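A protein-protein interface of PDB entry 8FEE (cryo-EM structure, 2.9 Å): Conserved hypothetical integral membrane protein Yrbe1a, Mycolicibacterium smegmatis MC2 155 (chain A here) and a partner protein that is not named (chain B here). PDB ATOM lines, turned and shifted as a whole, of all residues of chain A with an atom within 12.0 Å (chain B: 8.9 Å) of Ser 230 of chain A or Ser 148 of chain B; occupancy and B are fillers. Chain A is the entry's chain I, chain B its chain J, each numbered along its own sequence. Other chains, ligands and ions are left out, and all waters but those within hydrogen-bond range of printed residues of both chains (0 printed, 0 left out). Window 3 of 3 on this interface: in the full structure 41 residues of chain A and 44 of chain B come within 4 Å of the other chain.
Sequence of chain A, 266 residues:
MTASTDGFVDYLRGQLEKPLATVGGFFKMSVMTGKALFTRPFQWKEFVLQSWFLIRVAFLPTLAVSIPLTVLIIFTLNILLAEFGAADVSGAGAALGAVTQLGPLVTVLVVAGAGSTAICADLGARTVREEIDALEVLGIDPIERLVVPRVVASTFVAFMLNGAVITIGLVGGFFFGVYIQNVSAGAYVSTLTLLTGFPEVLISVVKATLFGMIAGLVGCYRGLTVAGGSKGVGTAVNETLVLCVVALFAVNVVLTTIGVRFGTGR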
ATOM      1  N   ALA A 121      13.486 -24.385  -7.559  1.00  0.00           N
ATOM      2  CA  ALA A 121      13.197 -23.977  -8.929  1.00  0.00           C
ATOM      3  C   ALA A 121      13.298 -22.467  -9.095  1.00  0.00           C
ATOM      4  O   ALA A 121      13.834 -21.984 -10.097  1.00  0.00           O
ATOM      5  CB  ALA A 121      11.811 -24.469  -9.340  1.00  0.00           C
ATOM      6  N   GLY A 124      16.964 -21.454  -8.943  1.00  0.00           N
ATOM      7  CA  GLY A 124      17.601 -21.865 -10.184  1.00  0.00           C
ATOM      8  C   GLY A 124      17.219 -20.975 -11.351  1.00  0.00           C
ATOM      9  O   GLY A 124      18.053 -20.672 -12.211  1.00  0.00           O
ATOM     10  N   ALA A 125      15.956 -20.545 -11.397  1.00  0.00           N
ATOM     11  CA  ALA A 125      15.518 -19.606 -12.424  1.00  0.00           C
ATOM     12  C   ALA A 125      16.251 -18.279 -12.302  1.00  0.00           C
ATOM     13  O   ALA A 125      16.666 -17.696 -13.310  1.00  0.00           O
ATOM     14  CB  ALA A 125      14.009 -19.391 -12.327  1.00  0.00           C
ATOM     15  N   THR A 127      19.207 -17.916 -10.997  1.00  0.00           N
ATOM     16  CA  THR A 127      20.615 -18.150 -11.299  1.00  0.00           C
ATOM     17  C   THR A 127      20.859 -18.222 -12.804  1.00  0.00           C
ATOM     18  O   THR A 127      21.799 -17.605 -13.318  1.00  0.00           O
ATOM     19  CB  THR A 127      21.094 -19.429 -10.613  1.00  0.00           C
ATOM     20  OG1 THR A 127      21.040 -19.258  -9.192  1.00  0.00           O
ATOM     21  CG2 THR A 127      22.525 -19.743 -11.013  1.00  0.00           C
ATOM     22  N   VAL A 128      20.023 -18.971 -13.530  1.00  0.00           N
ATOM     23  CA  VAL A 128      20.236 -19.116 -14.969  1.00  0.00           C
ATOM     24  C   VAL A 128      19.925 -17.820 -15.710  1.00  0.00           C
ATOM     25  O   VAL A 128      20.469 -17.576 -16.793  1.00  0.00           O
ATOM     26  CB  VAL A 128      19.414 -20.293 -15.530  1.00  0.00           C
ATOM     27  CG1 VAL A 128      19.819 -21.591 -14.854  1.00  0.00           C
ATOM     28  CG2 VAL A 128      17.922 -20.039 -15.378  1.00  0.00           C
ATOM     29  N   ARG A 129      19.063 -16.973 -15.157  1.00  0.00           N
ATOM     30  CA  ARG A 129      18.791 -15.668 -15.745  1.00  0.00           C
ATOM     31  C   ARG A 129      19.790 -14.610 -15.302  1.00  0.00           C
ATOM     32  O   ARG A 129      19.608 -13.434 -15.637  1.00  0.00           O
ATOM     33  CB  ARG A 129      17.369 -15.211 -15.408  1.00  0.00           C
ATOM     34  CG  ARG A 129      16.279 -16.073 -16.018  1.00  0.00           C
ATOM     35  CD  ARG A 129      14.901 -15.589 -15.603  1.00  0.00           C
ATOM     36  NE  ARG A 129      13.847 -16.480 -16.074  1.00  0.00           N
ATOM     37  CZ  ARG A 129      12.561 -16.334 -15.789  1.00  0.00           C
ATOM     38  NH1 ARG A 129      12.128 -15.336 -15.037  1.00  0.00           N
ATOM     39  NH2 ARG A 129      11.686 -17.212 -16.272  1.00  0.00           N
ATOM     40  N   ARG A 222      20.504 -25.673  -3.100  1.00  0.00           N
ATOM     41  CA  ARG A 222      20.494 -26.292  -4.420  1.00  0.00           C
ATOM     42  C   ARG A 222      20.074 -25.310  -5.504  1.00  0.00           C
ATOM     43  O   ARG A 222      20.543 -25.411  -6.643  1.00  0.00           O
ATOM     44  CB  ARG A 222      19.583 -27.514  -4.429  1.00  0.00           C
ATOM     45  CG  ARG A 222      20.199 -28.760  -3.818  1.00  0.00           C
ATOM     46  CD  ARG A 222      21.492 -29.135  -4.522  1.00  0.00           C
ATOM     47  NE  ARG A 222      21.334 -29.184  -5.971  1.00  0.00           N
ATOM     48  CZ  ARG A 222      22.276 -29.586  -6.813  1.00  0.00           C
ATOM     49  NH1 ARG A 222      23.456 -30.004  -6.384  1.00  0.00           N
ATOM     50  NH2 ARG A 222      22.027 -29.572  -8.119  1.00  0.00           N
ATOM     51  N   VAL A 226      22.721 -24.150  -9.166  1.00  0.00           N
ATOM     52  CA  VAL A 226      22.139 -24.863 -10.297  1.00  0.00           C
ATOM     53  C   VAL A 226      23.140 -24.887 -11.446  1.00  0.00           C
ATOM     54  O   VAL A 226      24.005 -24.012 -11.569  1.00  0.00           O
ATOM     55  CB  VAL A 226      20.794 -24.227 -10.710  1.00  0.00           C
ATOM     56  CG1 VAL A 226      21.008 -23.024 -11.603  1.00  0.00           C
ATOM     57  CG2 VAL A 226      19.909 -25.250 -11.394  1.00  0.00           C
ATOM     58  N   ALA A 227      23.042 -25.919 -12.281  1.00  0.00           N
ATOM     59  CA  ALA A 227      24.036 -26.188 -13.312  1.00  0.00           C
ATOM     60  C   ALA A 227      23.703 -25.551 -14.655  1.00  0.00           C
ATOM     61  O   ALA A 227      24.472 -25.721 -15.607  1.00  0.00           O
ATOM     62  CB  ALA A 227      24.208 -27.699 -13.494  1.00  0.00           C
ATOM     63  N   GLY A 228      22.596 -24.817 -14.752  1.00  0.00           N
ATOM     64  CA  GLY A 228      22.235 -24.183 -16.009  1.00  0.00           C
ATOM     65  C   GLY A 228      21.935 -25.211 -17.081  1.00  0.00           C
ATOM     66  O   GLY A 228      21.349 -26.264 -16.817  1.00  0.00           O
ATOM     67  N   GLY A 229      22.357 -24.916 -18.307  1.00  0.00           N
ATOM     68  CA  GLY A 229      22.089 -25.829 -19.403  1.00  0.00           C
ATOM     69  C   GLY A 229      20.603 -25.982 -19.674  1.00  0.00           C
ATOM     70  O   GLY A 229      19.810 -25.046 -19.525  1.00  0.00           O
ATOM     71  N   SER A 230      20.217 -27.195 -20.077  1.00  0.00           N
ATOM     72  CA  SER A 230      18.828 -27.505 -20.384  1.00  0.00           C
ATOM     73  C   SER A 230      18.182 -28.478 -19.410  1.00  0.00           C
ATOM     74  O   SER A 230      16.950 -28.528 -19.345  1.00  0.00           O
ATOM     75  CB  SER A 230      18.712 -28.080 -21.804  1.00  0.00           C
ATOM     76  OG  SER A 230      17.363 -28.369 -22.124  1.00  0.00           O
ATOM     77  N   LYS A 231      18.970 -29.245 -18.657  1.00  0.00           N
ATOM     78  CA  LYS A 231      18.444 -30.156 -17.647  1.00  0.00           C
ATOM     79  C   LYS A 231      18.943 -29.806 -16.248  1.00  0.00           C
ATOM     80  O   LYS A 231      18.737 -30.584 -15.310  1.00  0.00           O
ATOM     81  CB  LYS A 231      18.819 -31.599 -18.005  1.00  0.00           C
ATOM     82  CG  LYS A 231      17.917 -32.674 -17.411  1.00  0.00           C
ATOM     83  CD  LYS A 231      18.457 -34.061 -17.705  1.00  0.00           C
ATOM     84  CE  LYS A 231      17.721 -35.118 -16.903  1.00  0.00           C
ATOM     85  NZ  LYS A 231      18.354 -36.454 -17.053  1.00  0.00           N
ATOM     86  N   GLY A 232      19.592 -28.653 -16.085  1.00  0.00           N
ATOM     87  CA  GLY A 232      20.144 -28.301 -14.788  1.00  0.00           C
ATOM     88  C   GLY A 232      19.089 -28.040 -13.732  1.00  0.00           C
ATOM     89  O   GLY A 232      19.213 -28.502 -12.595  1.00  0.00           O
ATOM     90  N   VAL A 233      18.041 -27.294 -14.085  1.00  0.00           N
ATOM     91  CA  VAL A 233      17.021 -26.947 -13.100  1.00  0.00           C
ATOM     92  C   VAL A 233      16.204 -28.175 -12.710  1.00  0.00           C
ATOM     93  O   VAL A 233      15.870 -28.363 -11.535  1.00  0.00           O
ATOM     94  CB  VAL A 233      16.129 -25.813 -13.634  1.00  0.00           C
ATOM     95  CG1 VAL A 233      15.135 -25.374 -12.576  1.00  0.00           C
ATOM     96  CG2 VAL A 233      16.981 -24.642 -14.081  1.00  0.00           C
ATOM     97  N   GLY A 234      15.875 -29.032 -13.680  1.00  0.00           N
ATOM     98  CA  GLY A 234      15.138 -30.244 -13.355  1.00  0.00           C
ATOM     99  C   GLY A 234      15.923 -31.186 -12.464  1.00  0.00           C
ATOM    100  O   GLY A 234      15.389 -31.730 -11.490  1.00  0.00           O
ATOM    101  N   THR A 235      17.206 -31.384 -12.777  1.00  0.00           N
ATOM    102  CA  THR A 235      18.064 -32.203 -11.929  1.00  0.00           C
ATOM    103  C   THR A 235      18.208 -31.587 -10.544  1.00  0.00           C
ATOM    104  O   THR A 235      18.198 -32.301  -9.533  1.00  0.00           O
ATOM    105  CB  THR A 235      19.433 -32.381 -12.589  1.00  0.00           C
ATOM    106  OG1 THR A 235      19.288 -33.154 -13.785  1.00  0.00           O
ATOM    107  CG2 THR A 235      20.402 -33.092 -11.656  1.00  0.00           C
ATOM    108  N   ALA A 236      18.332 -30.258 -10.480  1.00  0.00           N
ATOM    109  CA  ALA A 236      18.440 -29.582  -9.193  1.00  0.00           C
ATOM    110  C   ALA A 236      17.194 -29.805  -8.349  1.00  0.00           C
ATOM    111  O   ALA A 236      17.294 -30.087  -7.152  1.00  0.00           O
ATOM    112  CB  ALA A 236      18.686 -28.090  -9.402  1.00  0.00           C
ATOM    113  N   VAL A 237      16.010 -29.689  -8.955  1.00  0.00           N
ATOM    114  CA  VAL A 237      14.769 -29.885  -8.211  1.00  0.00           C
ATOM    115  C   VAL A 237      14.635 -31.332  -7.750  1.00  0.00           C
ATOM    116  O   VAL A 237      14.226 -31.601  -6.612  1.00  0.00           O
ATOM    117  CB  VAL A 237      13.564 -29.440  -9.058  1.00  0.00           C
ATOM    118  CG1 VAL A 237      12.270 -29.778  -8.357  1.00  0.00           C
ATOM    119  CG2 VAL A 237      13.627 -27.949  -9.313  1.00  0.00           C
ATOM    120  N   ASN A 238      14.979 -32.288  -8.619  1.00  0.00           N
ATOM    121  CA  ASN A 238      14.891 -33.696  -8.241  1.00  0.00           C
ATOM    122  C   ASN A 238      15.827 -34.018  -7.077  1.00  0.00           C
ATOM    123  O   ASN A 238      15.431 -34.679  -6.105  1.00  0.00           O
ATOM    124  CB  ASN A 238      15.201 -34.575  -9.454  1.00  0.00           C
ATOM    125  CG  ASN A 238      15.012 -36.051  -9.175  1.00  0.00           C
ATOM    126  OD1 ASN A 238      14.378 -36.437  -8.193  1.00  0.00           O
ATOM    127  ND2 ASN A 238      15.552 -36.888 -10.050  1.00  0.00           N
ATOM    128  N   ALA B 140      11.870 -35.092 -15.387  1.00  0.00           N
ATOM    129  CA  ALA B 140      13.012 -34.293 -15.811  1.00  0.00           C
ATOM    130  C   ALA B 140      13.525 -34.740 -17.172  1.00  0.00           C
ATOM    131  O   ALA B 140      13.833 -33.904 -18.027  1.00  0.00           O
ATOM    132  CB  ALA B 140      14.124 -34.372 -14.765  1.00  0.00           C
ATOM    133  N   GLU B 141      13.625 -36.055 -17.392  1.00  0.00           N
ATOM    134  CA  GLU B 141      14.109 -36.557 -18.677  1.00  0.00           C
ATOM    135  C   GLU B 141      13.179 -36.154 -19.813  1.00  0.00           C
ATOM    136  O   GLU B 141      13.631 -35.686 -20.866  1.00  0.00           O
ATOM    137  CB  GLU B 141      14.255 -38.078 -18.622  1.00  0.00           C
ATOM    138  CG  GLU B 141      15.560 -38.565 -18.020  1.00  0.00           C
ATOM    139  CD  GLU B 141      16.742 -38.383 -18.952  1.00  0.00           C
ATOM    140  OE1 GLU B 141      16.522 -38.166 -20.162  1.00  0.00           O
ATOM    141  OE2 GLU B 141      17.893 -38.455 -18.473  1.00  0.00           O
ATOM    142  N   LEU B 142      11.869 -36.324 -19.618  1.00  0.00           N
ATOM    143  CA  LEU B 142      10.928 -35.997 -20.683  1.00  0.00           C
ATOM    144  C   LEU B 142      10.864 -34.494 -20.927  1.00  0.00           C
ATOM    145  O   LEU B 142      10.747 -34.056 -22.075  1.00  0.00           O
ATOM    146  CB  LEU B 142       9.544 -36.559 -20.359  1.00  0.00           C
ATOM    147  CG  LEU B 142       9.404 -38.081 -20.276  1.00  0.00           C
ATOM    148  CD1 LEU B 142       7.947 -38.485 -20.415  1.00  0.00           C
ATOM    149  CD2 LEU B 142      10.256 -38.776 -21.326  1.00  0.00           C
ATOM    150  N   GLY B 143      10.949 -33.687 -19.866  1.00  0.00           N
ATOM    151  CA  GLY B 143      11.002 -32.246 -20.051  1.00  0.00           C
ATOM    152  C   GLY B 143      12.258 -31.797 -20.772  1.00  0.00           C
ATOM    153  O   GLY B 143      12.216 -30.889 -21.603  1.00  0.00           O
ATOM    154  N   ALA B 144      13.395 -32.426 -20.461  1.00  0.00           N
ATOM    155  CA  ALA B 144      14.635 -32.108 -21.159  1.00  0.00           C
ATOM    156  C   ALA B 144      14.545 -32.475 -22.632  1.00  0.00           C
ATOM    157  O   ALA B 144      15.018 -31.726 -23.495  1.00  0.00           O
ATOM    158  CB  ALA B 144      15.809 -32.827 -20.497  1.00  0.00           C
ATOM    159  N   MET B 145      13.951 -33.631 -22.940  1.00  0.00           N
ATOM    160  CA  MET B 145      13.774 -34.016 -24.337  1.00  0.00           C
ATOM    161  C   MET B 145      12.826 -33.064 -25.057  1.00  0.00           C
ATOM    162  O   MET B 145      13.055 -32.717 -26.221  1.00  0.00           O
ATOM    163  CB  MET B 145      13.267 -35.454 -24.427  1.00  0.00           C
ATOM    164  CG  MET B 145      14.319 -36.494 -24.094  1.00  0.00           C
ATOM    165  SD  MET B 145      13.755 -38.178 -24.381  1.00  0.00           S
ATOM    166  CE  MET B 145      15.260 -39.093 -24.061  1.00  0.00           C
ATOM    167  N   ARG B 146      11.751 -32.644 -24.387  1.00  0.00           N
ATOM    168  CA  ARG B 146      10.824 -31.688 -24.984  1.00  0.00           C
ATOM    169  C   ARG B 146      11.505 -30.352 -25.258  1.00  0.00           C
ATOM    170  O   ARG B 146      11.282 -29.736 -26.307  1.00  0.00           O
ATOM    171  CB  ARG B 146       9.613 -31.502 -24.070  1.00  0.00           C
ATOM    172  CG  ARG B 146       8.738 -30.313 -24.415  1.00  0.00           C
ATOM    173  CD  ARG B 146       7.997 -30.532 -25.719  1.00  0.00           C
ATOM    174  NE  ARG B 146       7.036 -31.624 -25.627  1.00  0.00           N
ATOM    175  CZ  ARG B 146       6.276 -32.038 -26.631  1.00  0.00           C
ATOM    176  NH1 ARG B 146       6.346 -31.476 -27.827  1.00  0.00           N
ATOM    177  NH2 ARG B 146       5.426 -33.040 -26.431  1.00  0.00           N
ATOM    178  N   ILE B 147      12.344 -29.891 -24.328  1.00  0.00           N
ATOM    179  CA  ILE B 147      13.046 -28.625 -24.514  1.00  0.00           C
ATOM    180  C   ILE B 147      14.115 -28.756 -25.592  1.00  0.00           C
ATOM    181  O   ILE B 147      14.251 -27.885 -26.460  1.00  0.00           O
ATOM    182  CB  ILE B 147      13.636 -28.142 -23.176  1.00  0.00           C
ATOM    183  CG1 ILE B 147      12.514 -27.752 -22.210  1.00  0.00           C
ATOM    184  CG2 ILE B 147      14.583 -26.975 -23.390  1.00  0.00           C
ATOM    185  CD1 ILE B 147      11.426 -26.907 -22.840  1.00  0.00           C
ATOM    186  N   SER B 148      14.878 -29.849 -25.569  1.00  0.00           N
ATOM    187  CA  SER B 148      15.938 -30.063 -26.548  1.00  0.00           C
ATOM    188  C   SER B 148      15.410 -30.443 -27.925  1.00  0.00           C
ATOM    189  O   SER B 148      16.223 -30.713 -28.817  1.00  0.00           O
ATOM    190  CB  SER B 148      16.902 -31.144 -26.057  1.00  0.00           C
ATOM    191  OG  SER B 148      17.511 -30.769 -24.835  1.00  0.00           O
ATOM    192  N   GLU B 149      14.086 -30.478 -28.106  1.00  0.00           N
ATOM    193  CA  GLU B 149      13.453 -30.808 -29.384  1.00  0.00           C
ATOM    194  C   GLU B 149      13.850 -32.200 -29.868  1.00  0.00           C
ATOM    195  O   GLU B 149      14.098 -32.417 -31.055  1.00  0.00           O
ATOM    196  CB  GLU B 149      13.759 -29.751 -30.448  1.00  0.00           C
ATOM    197  CG  GLU B 149      12.986 -28.457 -30.267  1.00  0.00           C
ATOM    198  CD  GLU B 149      13.555 -27.319 -31.090  1.00  0.00           C
ATOM    199  OE1 GLU B 149      14.710 -27.439 -31.549  1.00  0.00           O
ATOM    200  OE2 GLU B 149      12.849 -26.307 -31.277  1.00  0.00           O
ATOM    201  N   GLU B 150      13.920 -33.152 -28.939  1.00  0.00           N
ATOM    202  CA  GLU B 150      14.101 -34.548 -29.311  1.00  0.00           C
ATOM    203  C   GLU B 150      12.779 -35.268 -29.529  1.00  0.00           C
ATOM    204  O   GLU B 150      12.752 -36.284 -30.231  1.00  0.00           O
ATOM    205  CB  GLU B 150      14.917 -35.275 -28.240  1.00  0.00           C
ATOM    206  CG  GLU B 150      16.311 -34.702 -28.047  1.00  0.00           C
ATOM    207  CD  GLU B 150      17.056 -35.346 -26.897  1.00  0.00           C
ATOM    208  OE1 GLU B 150      16.764 -36.515 -26.574  1.00  0.00           O
ATOM    209  OE2 GLU B 150      17.938 -34.682 -26.312  1.00  0.00           O
ATOM    210  N   VAL B 151      11.685 -34.757 -28.959  1.00  0.00           N
ATOM    211  CA  VAL B 151      10.354 -35.242 -29.317  1.00  0.00           C
ATOM    212  C   VAL B 151      10.054 -34.910 -30.773  1.00  0.00           C
ATOM    213  O   VAL B 151       9.542 -35.747 -31.530  1.00  0.00           O
ATOM    214  CB  VAL B 151       9.299 -34.650 -28.363  1.00  0.00           C
ATOM    215  CG1 VAL B 151       7.905 -34.766 -28.957  1.00  0.00           C
ATOM    216  CG2 VAL B 151       9.362 -35.343 -27.012  1.00  0.00           C
ATOM    217  N   ASP B 152      10.376 -33.683 -31.189  1.00  0.00           N
ATOM    218  CA  ASP B 152      10.241 -33.311 -32.591  1.00  0.00           C
ATOM    219  C   ASP B 152      11.175 -34.131 -33.470  1.00  0.00           C
ATOM    220  O   ASP B 152      10.816 -34.493 -34.594  1.00  0.00           O
ATOM    221  CB  ASP B 152      10.512 -31.817 -32.767  1.00  0.00           C
ATOM    222  CG  ASP B 152       9.389 -30.955 -32.228  1.00  0.00           C
ATOM    223  OD1 ASP B 152       8.431 -31.516 -31.657  1.00  0.00           O
ATOM    224  OD2 ASP B 152       9.463 -29.718 -32.374  1.00  0.00           O
ATOM    225  N   ALA B 153      12.381 -34.425 -32.980  1.00  0.00           N
ATOM    226  CA  ALA B 153      13.295 -35.280 -33.731  1.00  0.00           C
ATOM    227  C   ALA B 153      12.710 -36.674 -33.928  1.00  0.00           C
ATOM    228  O   ALA B 153      12.850 -37.267 -35.004  1.00  0.00           O
ATOM    229  CB  ALA B 153      14.645 -35.362 -33.021  1.00  0.00           C
ATOM    230  N   LEU B 154      12.053 -37.213 -32.898  1.00  0.00           N
ATOM    231  CA  LEU B 154      11.401 -38.514 -33.022  1.00  0.00           C
ATOM    232  C   LEU B 154      10.243 -38.466 -34.010  1.00  0.00           C
ATOM    233  O   LEU B 154      10.080 -39.378 -34.827  1.00  0.00           O
ATOM    234  CB  LEU B 154      10.912 -38.987 -31.655  1.00  0.00           C
ATOM    235  CG  LEU B 154      11.977 -39.484 -30.684  1.00  0.00           C
ATOM    236  CD1 LEU B 154      11.335 -39.883 -29.368  1.00  0.00           C
ATOM    237  CD2 LEU B 154      12.731 -40.654 -31.291  1.00  0.00           C
ATOM    238  N   ALA B 245       5.964 -30.479 -21.167  1.00  0.00           N
ATOM    239  CA  ALA B 245       6.675 -29.393 -20.508  1.00  0.00           C
ATOM    240  C   ALA B 245       6.811 -28.197 -21.443  1.00  0.00           C
ATOM    241  O   ALA B 245       6.794 -28.332 -22.670  1.00  0.00           O
ATOM    242  CB  ALA B 245       8.055 -29.859 -20.047  1.00  0.00           C
ATOM    243  N   GLY B 247       8.342 -23.738 -21.439  1.00  0.00           N
ATOM    244  CA  GLY B 247       9.012 -22.654 -20.752  1.00  0.00           C
ATOM    245  C   GLY B 247      10.504 -22.810 -20.589  1.00  0.00           C
ATOM    246  O   GLY B 247      11.076 -22.205 -19.676  1.00  0.00           O
ATOM    247  N   GLY B 248      11.157 -23.597 -21.441  1.00  0.00           N
ATOM    248  CA  GLY B 248      12.594 -23.734 -21.332  1.00  0.00           C
ATOM    249  C   GLY B 248      12.988 -24.583 -20.133  1.00  0.00           C
ATOM    250  O   GLY B 248      12.187 -25.326 -19.562  1.00  0.00           O
ATOM    251  N   ALA B 249      14.264 -24.463 -19.758  1.00  0.00           N
ATOM    252  CA  ALA B 249      14.798 -25.232 -18.640  1.00  0.00           C
ATOM    253  C   ALA B 249      14.168 -24.842 -17.308  1.00  0.00           C
ATOM    254  O   ALA B 249      14.199 -25.639 -16.367  1.00  0.00           O
ATOM    255  CB  ALA B 249      16.315 -25.066 -18.564  1.00  0.00           C
ATOM    256  N   VAL B 250      13.605 -23.636 -17.209  1.00  0.00           N
ATOM    257  CA  VAL B 250      12.947 -23.215 -15.978  1.00  0.00           C
ATOM    258  C   VAL B 250      11.666 -24.010 -15.747  1.00  0.00           C
ATOM    259  O   VAL B 250      11.355 -24.395 -14.614  1.00  0.00           O
ATOM    260  CB  VAL B 250      12.672 -21.701 -16.023  1.00  0.00           C
ATOM    261  CG1 VAL B 250      11.998 -21.241 -14.743  1.00  0.00           C
ATOM    262  CG2 VAL B 250      13.964 -20.936 -16.259  1.00  0.00           C
ATOM    263  N   GLY B 251      10.910 -24.277 -16.815  1.00  0.00           N
ATOM    264  CA  GLY B 251       9.622 -24.940 -16.684  1.00  0.00           C
ATOM    265  C   GLY B 251       9.701 -26.387 -16.241  1.00  0.00           C
ATOM    266  O   GLY B 251       8.714 -26.916 -15.717  1.00  0.00           O
ATOM    267  N   VAL B 252      10.852 -27.033 -16.432  1.00  0.00           N
ATOM    268  CA  VAL B 252      11.012 -28.420 -16.005  1.00  0.00           C
ATOM    269  C   VAL B 252      10.888 -28.539 -14.490  1.00  0.00           C
ATOM    270  O   VAL B 252      10.288 -29.491 -13.978  1.00  0.00           O
ATOM    271  CB  VAL B 252      12.354 -28.980 -16.512  1.00  0.00           C
ATOM    272  CG1 VAL B 252      12.456 -30.467 -16.223  1.00  0.00           C
ATOM    273  CG2 VAL B 252      12.508 -28.713 -17.999  1.00  0.00           C
ATOM    274  N   GLY B 253      11.438 -27.574 -13.750  1.00  0.00           N
ATOM    275  CA  GLY B 253      11.330 -27.621 -12.298  1.00  0.00           C
ATOM    276  C   GLY B 253       9.899 -27.496 -11.809  1.00  0.00           C
ATOM    277  O   GLY B 253       9.474 -28.218 -10.900  1.00  0.00           O
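NZ of Lys 231 of chain A is in salt-bridge range of OE2 of Glu 141 of chain B.
The backbone carbonyl oxygen (O) of Lys 231 of chain A sits at hydrogen-bond distance from the side-chain hydroxyl (OG1) of Thr 235 of chain A (3.0 Å).
OG of Ser 148 of chain B sits at hydrogen-bond distance from O of Ala 144 of chain B.
Ala 125 of chain A touches Val 250 of chain B.
O of Gly 229 of chain A touches CB of Ala 249 of chain B (3.6 Å).
Ile 147 of chain B touches Ser 230 of chain A (CG2 to OG, 3.4 Å).
Ser 230 of chain A touches Ser 148 of chain B (OG to OG, 3.6 Å).
Ser 230 of chain A touches Ala 249 of chain B.
Lys 231 of chain A touches Ala 144 of chain B (CG to CB, 3.7 Å).
O of Ala 249 of chain B touches CB of Val 233 of chain A, at 3.4 Å.
CA of Gly 234 of chain A touches CG1 of Val 252 of chain B, at 3.9 Å.
Val 237 of chain A touches Gly 253 of chain B (CG2 to CA, 3.8 Å).
Ser 230 of chain A touches three residues of chain B.
Ser 148 of chain B touches one residue of chain A.
Ala 144 of chain B touches just one residue of chain A: Lys 231 (3.7 Å).
Of the printed residues of chain A, Ile 147 of chain B touches Ser 230 (3.4 Å).
No residue of chain A comes within 4 Å of Glu 149 of chain B.
No residue of chain A comes within 4 Å of Gly 248 of chain B.
Ala 249 of chain B touches just these residues of chain A: Gly 229, Ser 230 and Val 233.
Printed residues of chain A within 4 Å of Glu 141 of chain B: Lys 231 (2.5 Å).
Printed residues of chain B within 4 Å of Lys 231 of chain A: Glu 141 and Ala 144.
Of the printed residues of chain B, Ala 125 of chain A touches Val 250.
Of the printed residues of chain B, Val 237 of chain A touches Gly 253 (3.8 Å).
Of the printed residues of chain A, Val 252 of chain B touches Gly 234.
Gly 232 of chain A touches none of the printed residues of chain B.
The nearest residue of chain B that does not touch Ser 230 of chain A is Ala 144 of chain B (4.3 Å).
The nearest printed residue of chain B that does not touch Lys 231 of chain A is Ala 140 of chain B (4.2 Å).
Of the 23 printed residues of chain B, 8 touch a printed residue of chain A.
Hydrophobic or aromatic side chains of chain B within 4 Å of the printed part of chain A: Ala 144, Ile 147, Ala 249, Val 250 and Val 252.
Hydrophobic or aromatic side chains of chain A within 4 Å of the printed part of chain B: Ala 125, Val 233 and Val 237.
Among the printed residues, Asp or Glu carboxylates within 4 Å of a Lys or Arg side-chain nitrogen of the other chain: Lys 231 of chain A with Glu 141 of chain B (2.5 Å).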
